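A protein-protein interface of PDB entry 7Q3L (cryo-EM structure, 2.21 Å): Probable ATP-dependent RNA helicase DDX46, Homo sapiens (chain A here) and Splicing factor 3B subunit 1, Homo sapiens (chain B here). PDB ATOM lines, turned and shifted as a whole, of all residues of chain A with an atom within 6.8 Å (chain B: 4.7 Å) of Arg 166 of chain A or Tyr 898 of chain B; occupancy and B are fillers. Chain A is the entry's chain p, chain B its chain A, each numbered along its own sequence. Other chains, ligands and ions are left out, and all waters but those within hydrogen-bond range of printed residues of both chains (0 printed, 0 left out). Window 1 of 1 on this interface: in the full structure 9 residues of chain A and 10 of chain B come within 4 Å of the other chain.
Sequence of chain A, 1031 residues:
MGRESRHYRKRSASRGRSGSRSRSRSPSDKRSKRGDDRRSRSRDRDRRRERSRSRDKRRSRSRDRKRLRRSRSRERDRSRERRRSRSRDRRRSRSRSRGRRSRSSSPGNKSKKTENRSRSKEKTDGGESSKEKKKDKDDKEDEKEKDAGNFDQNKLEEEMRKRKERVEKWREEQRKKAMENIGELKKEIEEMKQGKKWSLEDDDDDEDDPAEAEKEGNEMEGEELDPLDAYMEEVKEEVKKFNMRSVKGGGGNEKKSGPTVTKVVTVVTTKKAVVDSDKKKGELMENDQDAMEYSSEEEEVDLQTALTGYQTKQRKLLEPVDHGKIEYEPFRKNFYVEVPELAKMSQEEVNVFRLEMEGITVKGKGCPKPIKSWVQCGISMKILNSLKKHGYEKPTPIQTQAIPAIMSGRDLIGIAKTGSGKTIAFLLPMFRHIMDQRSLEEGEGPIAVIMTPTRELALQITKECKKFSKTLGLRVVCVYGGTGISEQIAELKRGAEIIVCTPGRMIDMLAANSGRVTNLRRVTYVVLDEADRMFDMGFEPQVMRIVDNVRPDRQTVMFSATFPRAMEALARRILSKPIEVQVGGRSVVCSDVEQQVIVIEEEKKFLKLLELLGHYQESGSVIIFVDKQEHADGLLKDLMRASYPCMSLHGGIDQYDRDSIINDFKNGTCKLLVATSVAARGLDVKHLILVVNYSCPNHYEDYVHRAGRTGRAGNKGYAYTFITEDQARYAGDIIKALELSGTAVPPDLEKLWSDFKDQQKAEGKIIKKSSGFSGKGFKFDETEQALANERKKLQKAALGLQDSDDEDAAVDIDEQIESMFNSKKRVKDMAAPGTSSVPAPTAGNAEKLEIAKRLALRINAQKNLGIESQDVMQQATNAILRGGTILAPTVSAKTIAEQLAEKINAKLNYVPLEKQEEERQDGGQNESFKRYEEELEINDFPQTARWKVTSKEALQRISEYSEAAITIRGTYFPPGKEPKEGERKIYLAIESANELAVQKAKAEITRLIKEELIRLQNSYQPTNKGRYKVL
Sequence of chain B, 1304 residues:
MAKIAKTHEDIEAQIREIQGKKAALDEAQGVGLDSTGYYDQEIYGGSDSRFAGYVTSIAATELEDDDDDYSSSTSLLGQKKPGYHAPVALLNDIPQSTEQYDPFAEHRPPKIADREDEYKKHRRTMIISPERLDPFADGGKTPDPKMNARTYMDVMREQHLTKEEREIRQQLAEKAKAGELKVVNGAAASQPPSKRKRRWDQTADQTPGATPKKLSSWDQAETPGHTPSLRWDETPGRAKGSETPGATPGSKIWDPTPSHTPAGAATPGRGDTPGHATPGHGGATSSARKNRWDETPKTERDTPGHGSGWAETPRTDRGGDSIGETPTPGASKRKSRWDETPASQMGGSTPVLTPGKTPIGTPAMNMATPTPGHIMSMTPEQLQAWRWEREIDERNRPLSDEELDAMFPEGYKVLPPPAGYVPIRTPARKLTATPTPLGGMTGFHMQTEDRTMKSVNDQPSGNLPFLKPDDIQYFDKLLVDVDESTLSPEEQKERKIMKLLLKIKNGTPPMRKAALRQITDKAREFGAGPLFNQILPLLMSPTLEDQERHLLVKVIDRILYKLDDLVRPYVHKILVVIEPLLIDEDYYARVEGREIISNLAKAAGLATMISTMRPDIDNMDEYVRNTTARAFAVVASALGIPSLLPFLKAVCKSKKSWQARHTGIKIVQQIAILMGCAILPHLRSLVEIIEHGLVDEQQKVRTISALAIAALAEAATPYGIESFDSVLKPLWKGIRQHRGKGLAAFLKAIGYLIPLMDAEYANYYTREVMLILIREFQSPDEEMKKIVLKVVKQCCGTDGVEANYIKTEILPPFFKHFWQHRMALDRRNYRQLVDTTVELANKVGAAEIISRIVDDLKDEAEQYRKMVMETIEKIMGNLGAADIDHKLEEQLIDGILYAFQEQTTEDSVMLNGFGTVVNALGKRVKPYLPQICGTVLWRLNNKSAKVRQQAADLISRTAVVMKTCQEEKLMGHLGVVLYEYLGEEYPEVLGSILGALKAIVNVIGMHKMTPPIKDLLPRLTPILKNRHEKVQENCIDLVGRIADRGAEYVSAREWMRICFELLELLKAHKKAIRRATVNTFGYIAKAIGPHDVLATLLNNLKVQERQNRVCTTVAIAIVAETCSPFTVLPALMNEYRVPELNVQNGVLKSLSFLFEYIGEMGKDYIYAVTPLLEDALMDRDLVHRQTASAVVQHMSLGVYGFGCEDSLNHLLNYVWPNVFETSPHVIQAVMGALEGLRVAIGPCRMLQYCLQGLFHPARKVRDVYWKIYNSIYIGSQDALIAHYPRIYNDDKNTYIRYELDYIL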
ATOM      1  N   ARG A 161       3.591   0.448  32.414  1.00  0.00           N
ATOM      2  CA  ARG A 161       4.177  -0.837  32.044  1.00  0.00           C
ATOM      3  C   ARG A 161       3.391  -1.488  30.902  1.00  0.00           C
ATOM      4  O   ARG A 161       3.968  -1.828  29.865  1.00  0.00           O
ATOM      5  CB  ARG A 161       4.341  -1.749  33.263  1.00  0.00           C
ATOM      6  CG  ARG A 161       5.412  -1.265  34.225  1.00  0.00           C
ATOM      7  CD  ARG A 161       5.463  -2.014  35.539  1.00  0.00           C
ATOM      8  NE  ARG A 161       6.657  -1.715  36.326  1.00  0.00           N
ATOM      9  CZ  ARG A 161       6.864  -0.626  37.070  1.00  0.00           C
ATOM     10  NH1 ARG A 161       8.003  -0.496  37.730  1.00  0.00           N
ATOM     11  NH2 ARG A 161       5.956   0.332  37.149  1.00  0.00           N
ATOM     12  N   LYS A 162       2.061  -1.578  31.059  1.00  0.00           N
ATOM     13  CA  LYS A 162       1.163  -2.105  30.038  1.00  0.00           C
ATOM     14  C   LYS A 162       1.069  -1.200  28.807  1.00  0.00           C
ATOM     15  O   LYS A 162       0.938  -1.715  27.699  1.00  0.00           O
ATOM     16  CB  LYS A 162      -0.217  -2.424  30.619  1.00  0.00           C
ATOM     17  CG  LYS A 162      -0.317  -3.759  31.348  1.00  0.00           C
ATOM     18  CD  LYS A 162      -0.169  -4.974  30.447  1.00  0.00           C
ATOM     19  CE  LYS A 162       0.017  -6.273  31.205  1.00  0.00           C
ATOM     20  NZ  LYS A 162       0.409  -7.383  30.302  1.00  0.00           N
ATOM     21  N   ARG A 163       1.179   0.125  28.976  1.00  0.00           N
ATOM     22  CA  ARG A 163       1.263   1.054  27.852  1.00  0.00           C
ATOM     23  C   ARG A 163       2.453   0.717  26.939  1.00  0.00           C
ATOM     24  O   ARG A 163       2.285   0.570  25.726  1.00  0.00           O
ATOM     25  CB  ARG A 163       1.249   2.499  28.371  1.00  0.00           C
ATOM     26  CG  ARG A 163       1.507   3.562  27.313  1.00  0.00           C
ATOM     27  CD  ARG A 163       0.501   3.573  26.169  1.00  0.00           C
ATOM     28  NE  ARG A 163       0.913   4.526  25.145  1.00  0.00           N
ATOM     29  CZ  ARG A 163       1.110   4.289  23.849  1.00  0.00           C
ATOM     30  NH1 ARG A 163       0.833   3.115  23.306  1.00  0.00           N
ATOM     31  NH2 ARG A 163       1.497   5.287  23.076  1.00  0.00           N
ATOM     32  N   LYS A 164       3.651   0.566  27.523  1.00  0.00           N
ATOM     33  CA  LYS A 164       4.875   0.243  26.794  1.00  0.00           C
ATOM     34  C   LYS A 164       4.795  -1.131  26.130  1.00  0.00           C
ATOM     35  O   LYS A 164       5.203  -1.279  24.978  1.00  0.00           O
ATOM     36  CB  LYS A 164       6.096   0.344  27.715  1.00  0.00           C
ATOM     37  CG  LYS A 164       6.463   1.755  28.160  1.00  0.00           C
ATOM     38  CD  LYS A 164       6.918   2.664  27.035  1.00  0.00           C
ATOM     39  CE  LYS A 164       7.265   4.062  27.500  1.00  0.00           C
ATOM     40  NZ  LYS A 164       7.691   4.919  26.369  1.00  0.00           N
ATOM     41  N   GLU A 165       4.227  -2.120  26.835  1.00  0.00           N
ATOM     42  CA  GLU A 165       3.955  -3.440  26.278  1.00  0.00           C
ATOM     43  C   GLU A 165       3.076  -3.373  25.023  1.00  0.00           C
ATOM     44  O   GLU A 165       3.413  -4.023  24.047  1.00  0.00           O
ATOM     45  CB  GLU A 165       3.367  -4.385  27.329  1.00  0.00           C
ATOM     46  CG  GLU A 165       4.383  -4.897  28.334  1.00  0.00           C
ATOM     47  CD  GLU A 165       3.902  -5.972  29.298  1.00  0.00           C
ATOM     48  OE1 GLU A 165       2.807  -6.533  29.081  1.00  0.00           O
ATOM     49  OE2 GLU A 165       4.632  -6.249  30.272  1.00  0.00           O
ATOM     50  N   ARG A 166       1.981  -2.596  25.017  1.00  0.00           N
ATOM     51  CA  ARG A 166       1.107  -2.482  23.847  1.00  0.00           C
ATOM     52  C   ARG A 166       1.865  -2.004  22.603  1.00  0.00           C
ATOM     53  O   ARG A 166       1.772  -2.629  21.542  1.00  0.00           O
ATOM     54  CB  ARG A 166      -0.094  -1.573  24.150  1.00  0.00           C
ATOM     55  CG  ARG A 166      -1.144  -1.448  23.049  1.00  0.00           C
ATOM     56  CD  ARG A 166      -2.035  -2.664  22.833  1.00  0.00           C
ATOM     57  NE  ARG A 166      -2.728  -3.017  24.063  1.00  0.00           N
ATOM     58  CZ  ARG A 166      -3.361  -4.151  24.330  1.00  0.00           C
ATOM     59  NH1 ARG A 166      -3.904  -4.295  25.522  1.00  0.00           N
ATOM     60  NH2 ARG A 166      -3.492  -5.113  23.434  1.00  0.00           N
ATOM     61  N   VAL A 167       2.607  -0.897  22.738  1.00  0.00           N
ATOM     62  CA  VAL A 167       3.263  -0.259  21.601  1.00  0.00           C
ATOM     63  C   VAL A 167       4.392  -1.131  21.035  1.00  0.00           C
ATOM     64  O   VAL A 167       4.485  -1.306  19.818  1.00  0.00           O
ATOM     65  CB  VAL A 167       3.677   1.204  21.885  1.00  0.00           C
ATOM     66  CG1 VAL A 167       4.617   1.359  23.073  1.00  0.00           C
ATOM     67  CG2 VAL A 167       4.254   1.888  20.656  1.00  0.00           C
ATOM     68  N   GLU A 168       5.214  -1.718  21.912  1.00  0.00           N
ATOM     69  CA  GLU A 168       6.309  -2.586  21.493  1.00  0.00           C
ATOM     70  C   GLU A 168       5.777  -3.891  20.890  1.00  0.00           C
ATOM     71  O   GLU A 168       6.283  -4.335  19.866  1.00  0.00           O
ATOM     72  CB  GLU A 168       7.325  -2.778  22.626  1.00  0.00           C
ATOM     73  CG  GLU A 168       6.914  -3.794  23.683  1.00  0.00           C
ATOM     74  CD  GLU A 168       7.752  -3.852  24.952  1.00  0.00           C
ATOM     75  OE1 GLU A 168       7.448  -4.700  25.812  1.00  0.00           O
ATOM     76  OE2 GLU A 168       8.728  -3.078  25.069  1.00  0.00           O
ATOM     77  N   LYS A 169       4.733  -4.469  21.499  1.00  0.00           N
ATOM     78  CA  LYS A 169       4.120  -5.725  21.083  1.00  0.00           C
ATOM     79  C   LYS A 169       3.603  -5.644  19.647  1.00  0.00           C
ATOM     80  O   LYS A 169       3.780  -6.602  18.897  1.00  0.00           O
ATOM     81  CB  LYS A 169       3.049  -6.145  22.096  1.00  0.00           C
ATOM     82  CG  LYS A 169       2.382  -7.499  21.876  1.00  0.00           C
ATOM     83  CD  LYS A 169       1.125  -7.432  21.032  1.00  0.00           C
ATOM     84  CE  LYS A 169       0.166  -8.559  21.359  1.00  0.00           C
ATOM     85  NZ  LYS A 169      -0.899  -8.712  20.343  1.00  0.00           N
ATOM     86  N   TRP A 170       3.009  -4.512  19.238  1.00  0.00           N
ATOM     87  CA  TRP A 170       2.704  -4.359  17.819  1.00  0.00           C
ATOM     88  C   TRP A 170       3.972  -4.268  16.960  1.00  0.00           C
ATOM     89  O   TRP A 170       4.082  -4.979  15.961  1.00  0.00           O
ATOM     90  CB  TRP A 170       1.702  -3.244  17.460  1.00  0.00           C
ATOM     91  CG  TRP A 170       1.598  -3.213  15.958  1.00  0.00           C
ATOM     92  CD1 TRP A 170       1.118  -4.242  15.196  1.00  0.00           C
ATOM     93  CD2 TRP A 170       2.123  -2.235  15.014  1.00  0.00           C
ATOM     94  NE1 TRP A 170       1.276  -3.964  13.864  1.00  0.00           N
ATOM     95  CE2 TRP A 170       1.906  -2.750  13.709  1.00  0.00           C
ATOM     96  CE3 TRP A 170       2.767  -0.987  15.111  1.00  0.00           C
ATOM     97  CZ2 TRP A 170       2.288  -2.052  12.546  1.00  0.00           C
ATOM     98  CZ3 TRP A 170       3.143  -0.296  13.968  1.00  0.00           C
ATOM     99  CH2 TRP A 170       2.911  -0.827  12.696  1.00  0.00           C
ATOM    100  N   ARG A 171       4.924  -3.397  17.312  1.00  0.00           N
ATOM    101  CA  ARG A 171       6.078  -3.192  16.440  1.00  0.00           C
ATOM    102  C   ARG A 171       6.999  -4.419  16.368  1.00  0.00           C
ATOM    103  O   ARG A 171       7.788  -4.529  15.432  1.00  0.00           O
ATOM    104  CB  ARG A 171       6.772  -1.861  16.742  1.00  0.00           C
ATOM    105  CG  ARG A 171       7.412  -1.179  15.537  1.00  0.00           C
ATOM    106  CD  ARG A 171       6.610  -1.234  14.242  1.00  0.00           C
ATOM    107  NE  ARG A 171       6.919  -0.195  13.271  1.00  0.00           N
ATOM    108  CZ  ARG A 171       8.011  -0.102  12.515  1.00  0.00           C
ATOM    109  NH1 ARG A 171       8.982  -0.997  12.597  1.00  0.00           N
ATOM    110  NH2 ARG A 171       8.124   0.912  11.679  1.00  0.00           N
ATOM    111  N   LEU B 857      -5.991  -1.829  12.006  1.00  0.00           N
ATOM    112  CA  LEU B 857      -6.156  -1.023  13.212  1.00  0.00           C
ATOM    113  C   LEU B 857      -4.813  -0.777  13.903  1.00  0.00           C
ATOM    114  O   LEU B 857      -4.650   0.246  14.563  1.00  0.00           O
ATOM    115  CB  LEU B 857      -7.106  -1.701  14.199  1.00  0.00           C
ATOM    116  CG  LEU B 857      -8.601  -1.468  14.004  1.00  0.00           C
ATOM    117  CD1 LEU B 857      -9.362  -2.432  14.894  1.00  0.00           C
ATOM    118  CD2 LEU B 857      -8.996  -0.034  14.343  1.00  0.00           C
ATOM    119  N   LYS B 858      -3.863  -1.707  13.747  1.00  0.00           N
ATOM    120  CA  LYS B 858      -2.556  -1.574  14.376  1.00  0.00           C
ATOM    121  C   LYS B 858      -1.539  -0.884  13.467  1.00  0.00           C
ATOM    122  O   LYS B 858      -0.356  -0.860  13.782  1.00  0.00           O
ATOM    123  CB  LYS B 858      -2.063  -2.936  14.866  1.00  0.00           C
ATOM    124  CG  LYS B 858      -2.985  -3.540  15.913  1.00  0.00           C
ATOM    125  CD  LYS B 858      -2.462  -4.783  16.589  1.00  0.00           C
ATOM    126  CE  LYS B 858      -2.546  -6.027  15.726  1.00  0.00           C
ATOM    127  NZ  LYS B 858      -2.206  -7.252  16.491  1.00  0.00           N
ATOM    128  N   ASP B 859      -1.987  -0.281  12.366  1.00  0.00           N
ATOM    129  CA  ASP B 859      -1.109   0.328  11.374  1.00  0.00           C
ATOM    130  C   ASP B 859      -0.297   1.518  11.914  1.00  0.00           C
ATOM    131  O   ASP B 859      -0.508   2.014  13.023  1.00  0.00           O
ATOM    132  CB  ASP B 859      -1.946   0.698  10.152  1.00  0.00           C
ATOM    133  CG  ASP B 859      -1.079   0.985   8.949  1.00  0.00           C
ATOM    134  OD1 ASP B 859      -0.572   0.018   8.354  1.00  0.00           O
ATOM    135  OD2 ASP B 859      -0.855   2.180   8.670  1.00  0.00           O
ATOM    136  N   ASP B 894      -7.394  -5.796  20.527  1.00  0.00           N
ATOM    137  CA  ASP B 894      -5.974  -5.452  20.510  1.00  0.00           C
ATOM    138  C   ASP B 894      -5.771  -4.190  19.666  1.00  0.00           C
ATOM    139  O   ASP B 894      -5.180  -3.218  20.142  1.00  0.00           O
ATOM    140  CB  ASP B 894      -5.103  -6.622  20.031  1.00  0.00           C
ATOM    141  CG  ASP B 894      -3.607  -6.338  19.978  1.00  0.00           C
ATOM    142  OD1 ASP B 894      -3.145  -5.437  20.715  1.00  0.00           O
ATOM    143  OD2 ASP B 894      -2.909  -7.033  19.219  1.00  0.00           O
ATOM    144  N   GLY B 895      -6.284  -4.212  18.427  1.00  0.00           N
ATOM    145  CA  GLY B 895      -6.149  -3.088  17.511  1.00  0.00           C
ATOM    146  C   GLY B 895      -6.824  -1.816  18.027  1.00  0.00           C
ATOM    147  O   GLY B 895      -6.250  -0.734  17.904  1.00  0.00           O
ATOM    148  N   ILE B 896      -8.032  -1.958  18.600  1.00  0.00           N
ATOM    149  CA  ILE B 896      -8.789  -0.819  19.118  1.00  0.00           C
ATOM    150  C   ILE B 896      -8.010  -0.148  20.256  1.00  0.00           C
ATOM    151  O   ILE B 896      -7.913   1.081  20.290  1.00  0.00           O
ATOM    152  CB  ILE B 896     -10.233  -1.224  19.507  1.00  0.00           C
ATOM    153  CG1 ILE B 896     -11.277  -0.635  18.556  1.00  0.00           C
ATOM    154  CG2 ILE B 896     -10.571  -0.899  20.955  1.00  0.00           C
ATOM    155  CD1 ILE B 896     -11.954  -1.656  17.681  1.00  0.00           C
ATOM    156  N   LEU B 897      -7.448  -0.963  21.167  1.00  0.00           N
ATOM    157  CA  LEU B 897      -6.656  -0.443  22.274  1.00  0.00           C
ATOM    158  C   LEU B 897      -5.405   0.258  21.746  1.00  0.00           C
ATOM    159  O   LEU B 897      -5.067   1.349  22.220  1.00  0.00           O
ATOM    160  CB  LEU B 897      -6.290  -1.583  23.231  1.00  0.00           C
ATOM    161  CG  LEU B 897      -7.450  -2.158  24.044  1.00  0.00           C
ATOM    162  CD1 LEU B 897      -7.044  -3.443  24.747  1.00  0.00           C
ATOM    163  CD2 LEU B 897      -7.973  -1.153  25.055  1.00  0.00           C
ATOM    164  N   TYR B 898      -4.741  -0.360  20.755  1.00  0.00           N
ATOM    165  CA  TYR B 898      -3.521   0.204  20.192  1.00  0.00           C
ATOM    166  C   TYR B 898      -3.810   1.555  19.535  1.00  0.00           C
ATOM    167  O   TYR B 898      -3.046   2.503  19.731  1.00  0.00           O
ATOM    168  CB  TYR B 898      -2.851  -0.752  19.198  1.00  0.00           C
ATOM    169  CG  TYR B 898      -1.512  -0.277  18.691  1.00  0.00           C
ATOM    170  CD1 TYR B 898      -1.356   0.218  17.405  1.00  0.00           C
ATOM    171  CD2 TYR B 898      -0.399  -0.285  19.517  1.00  0.00           C
ATOM    172  CE1 TYR B 898      -0.125   0.663  16.946  1.00  0.00           C
ATOM    173  CE2 TYR B 898       0.837   0.161  19.074  1.00  0.00           C
ATOM    174  CZ  TYR B 898       0.974   0.636  17.783  1.00  0.00           C
ATOM    175  OH  TYR B 898       2.187   1.081  17.350  1.00  0.00           O
ATOM    176  N   ALA B 899      -4.912   1.631  18.770  1.00  0.00           N
ATOM    177  CA  ALA B 899      -5.263   2.852  18.056  1.00  0.00           C
ATOM    178  C   ALA B 899      -5.529   3.992  19.040  1.00  0.00           C
ATOM    179  O   ALA B 899      -5.093   5.118  18.798  1.00  0.00           O
ATOM    180  CB  ALA B 899      -6.439   2.617  17.141  1.00  0.00           C
ATOM    181  N   PHE B 900      -6.227   3.685  20.146  1.00  0.00           N
ATOM    182  CA  PHE B 900      -6.566   4.686  21.154  1.00  0.00           C
ATOM    183  C   PHE B 900      -5.308   5.216  21.845  1.00  0.00           C
ATOM    184  O   PHE B 900      -5.198   6.423  22.082  1.00  0.00           O
ATOM    185  CB  PHE B 900      -7.572   4.130  22.168  1.00  0.00           C
ATOM    186  CG  PHE B 900      -8.649   5.095  22.597  1.00  0.00           C
ATOM    187  CD1 PHE B 900      -9.707   5.398  21.750  1.00  0.00           C
ATOM    188  CD2 PHE B 900      -8.605   5.704  23.844  1.00  0.00           C
ATOM    189  CE1 PHE B 900     -10.700   6.290  22.136  1.00  0.00           C
ATOM    190  CE2 PHE B 900      -9.591   6.605  24.227  1.00  0.00           C
ATOM    191  CZ  PHE B 900     -10.639   6.892  23.377  1.00  0.00           C
ATOM    192  N   GLN B 901      -4.365   4.315  22.154  1.00  0.00           N
ATOM    193  CA  GLN B 901      -3.122   4.694  22.816  1.00  0.00           C
ATOM    194  C   GLN B 901      -2.175   5.396  21.838  1.00  0.00           C
ATOM    195  O   GLN B 901      -1.210   6.028  22.280  1.00  0.00           O
ATOM    196  CB  GLN B 901      -2.444   3.461  23.418  1.00  0.00           C
ATOM    197  CG  GLN B 901      -3.060   2.993  24.729  1.00  0.00           C
ATOM    198  CD  GLN B 901      -2.734   1.557  25.066  1.00  0.00           C
ATOM    199  OE1 GLN B 901      -1.821   1.271  25.835  1.00  0.00           O
ATOM    200  NE2 GLN B 901      -3.490   0.635  24.492  1.00  0.00           N
ATOM    201  N   GLU B 902      -2.466   5.295  20.526  1.00  0.00           N
ATOM    202  CA  GLU B 902      -1.612   5.852  19.480  1.00  0.00           C
ATOM    203  C   GLU B 902      -1.997   7.269  19.043  1.00  0.00           C
ATOM    204  O   GLU B 902      -1.099   8.071  18.781  1.00  0.00           O
ATOM    205  CB  GLU B 902      -1.490   4.894  18.292  1.00  0.00           C
ATOM    206  CG  GLU B 902      -0.175   4.127  18.265  1.00  0.00           C
ATOM    207  CD  GLU B 902       0.497   3.915  19.611  1.00  0.00           C
ATOM    208  OE1 GLU B 902       1.572   4.504  19.827  1.00  0.00           O
ATOM    209  OE2 GLU B 902      -0.050   3.158  20.435  1.00  0.00           O
ATOM    210  N   GLN B 931      -7.613  -4.745  30.447  1.00  0.00           N
ATOM    211  CA  GLN B 931      -6.837  -4.059  29.420  1.00  0.00           C
ATOM    212  C   GLN B 931      -7.506  -2.743  29.014  1.00  0.00           C
ATOM    213  O   GLN B 931      -6.840  -1.721  28.842  1.00  0.00           O
ATOM    214  CB  GLN B 931      -6.676  -4.973  28.207  1.00  0.00           C
ATOM    215  CG  GLN B 931      -5.948  -6.275  28.511  1.00  0.00           C
ATOM    216  CD  GLN B 931      -5.688  -7.104  27.274  1.00  0.00           C
ATOM    217  OE1 GLN B 931      -5.269  -6.599  26.231  1.00  0.00           O
ATOM    218  NE2 GLN B 931      -5.924  -8.402  27.387  1.00  0.00           N
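OE1 of Gln 931 of chain B sits at hydrogen-bond distance from NH1 of Arg 166 of chain A, 2.8 Å away. O of Gln 901 of chain B sits at hydrogen-bond distance from NH2 of Arg 163 of chain A (2.9 Å). The side-chain carboxylate (OD1) of Asp 894 of chain B lies within salt-bridge range of the guanidinium group (NH2) of Arg 166 of chain A (2.8 Å). OE2 of Glu 902 of chain B lies within salt-bridge range of NH1 of Arg 163 of chain A, 3.0 Å away. The side-chain carboxylate (OD2) of Asp 894 of chain B lies within salt-bridge range of the side-chain amino group (NZ) of Lys 169 of chain A, 2.9 Å away.
The backbone carbonyl oxygen (O) of Leu 897 of chain B is in hydrogen-bond range of the side-chain amide nitrogen (NE2) of Gln 901 of chain B, at 2.9 Å. NZ of Lys 858 of chain B is in salt-bridge range of OD2 of Asp 894 of chain B (2.8 Å).
CD1 of Leu 897 of chain B touches NH1 of Arg 166 of chain A, at 3.3 Å. Arg 166 of chain A touches Tyr 898 of chain B. Arg 166 of chain A touches Gln 901 of chain B. Val 167 of chain A touches Tyr 898 of chain B. CG2 of Val 167 of chain A touches OE1 of Glu 902 of chain B, at 3.8 Å. CE2 of Trp 170 of chain A touches O of Lys 858 of chain B (2.9 Å). Trp 170 of chain A touches Tyr 898 of chain B.
Printed residues of chain B within 4 Å of Arg 166 of chain A: Asp 894, Leu 897, Tyr 898, Gln 901 and Gln 931. Gly 895 of chain B touches none of the printed residues of chain A. Tyr 898 of chain B touches just these residues of chain A: Arg 166, Val 167 and Trp 170. Printed residues of chain A within 4 Å of Glu 902 of chain B: Arg 163 (3.0 Å) and Val 167 (3.8 Å). Of the printed residues of chain A, Gln 931 of chain B touches Arg 166. The nearest residue of chain A that does not touch Tyr 898 of chain B is Arg 163 of chain A (5.2 Å). The nearest printed residue of chain B that does not touch Lys 169 of chain A is Lys 858 of chain B (4.3 Å).
Of the 11 printed residues of chain A, 5 touch a printed residue of chain B. Printed residues of chain A that touch a printed residue of chain B: Arg 163, Arg 166, Val 167, Lys 169 and Trp 170. Hydrophobic or aromatic side chains of chain B within 4 Å of the printed part of chain A: Leu 897 and Tyr 898. Among the printed residues, 12 pairs touch across the chains. Among the printed residues, Asp or Glu carboxylates within 4 Å of a Lys or Arg side-chain nitrogen of the other chain: Arg 163 of chain A with Glu 902 of chain B (3.0 Å), Arg 166 of chain A with Asp 894 of chain B (2.8 Å) and Lys 169 of chain A with Asp 894 of chain B (2.9 Å).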
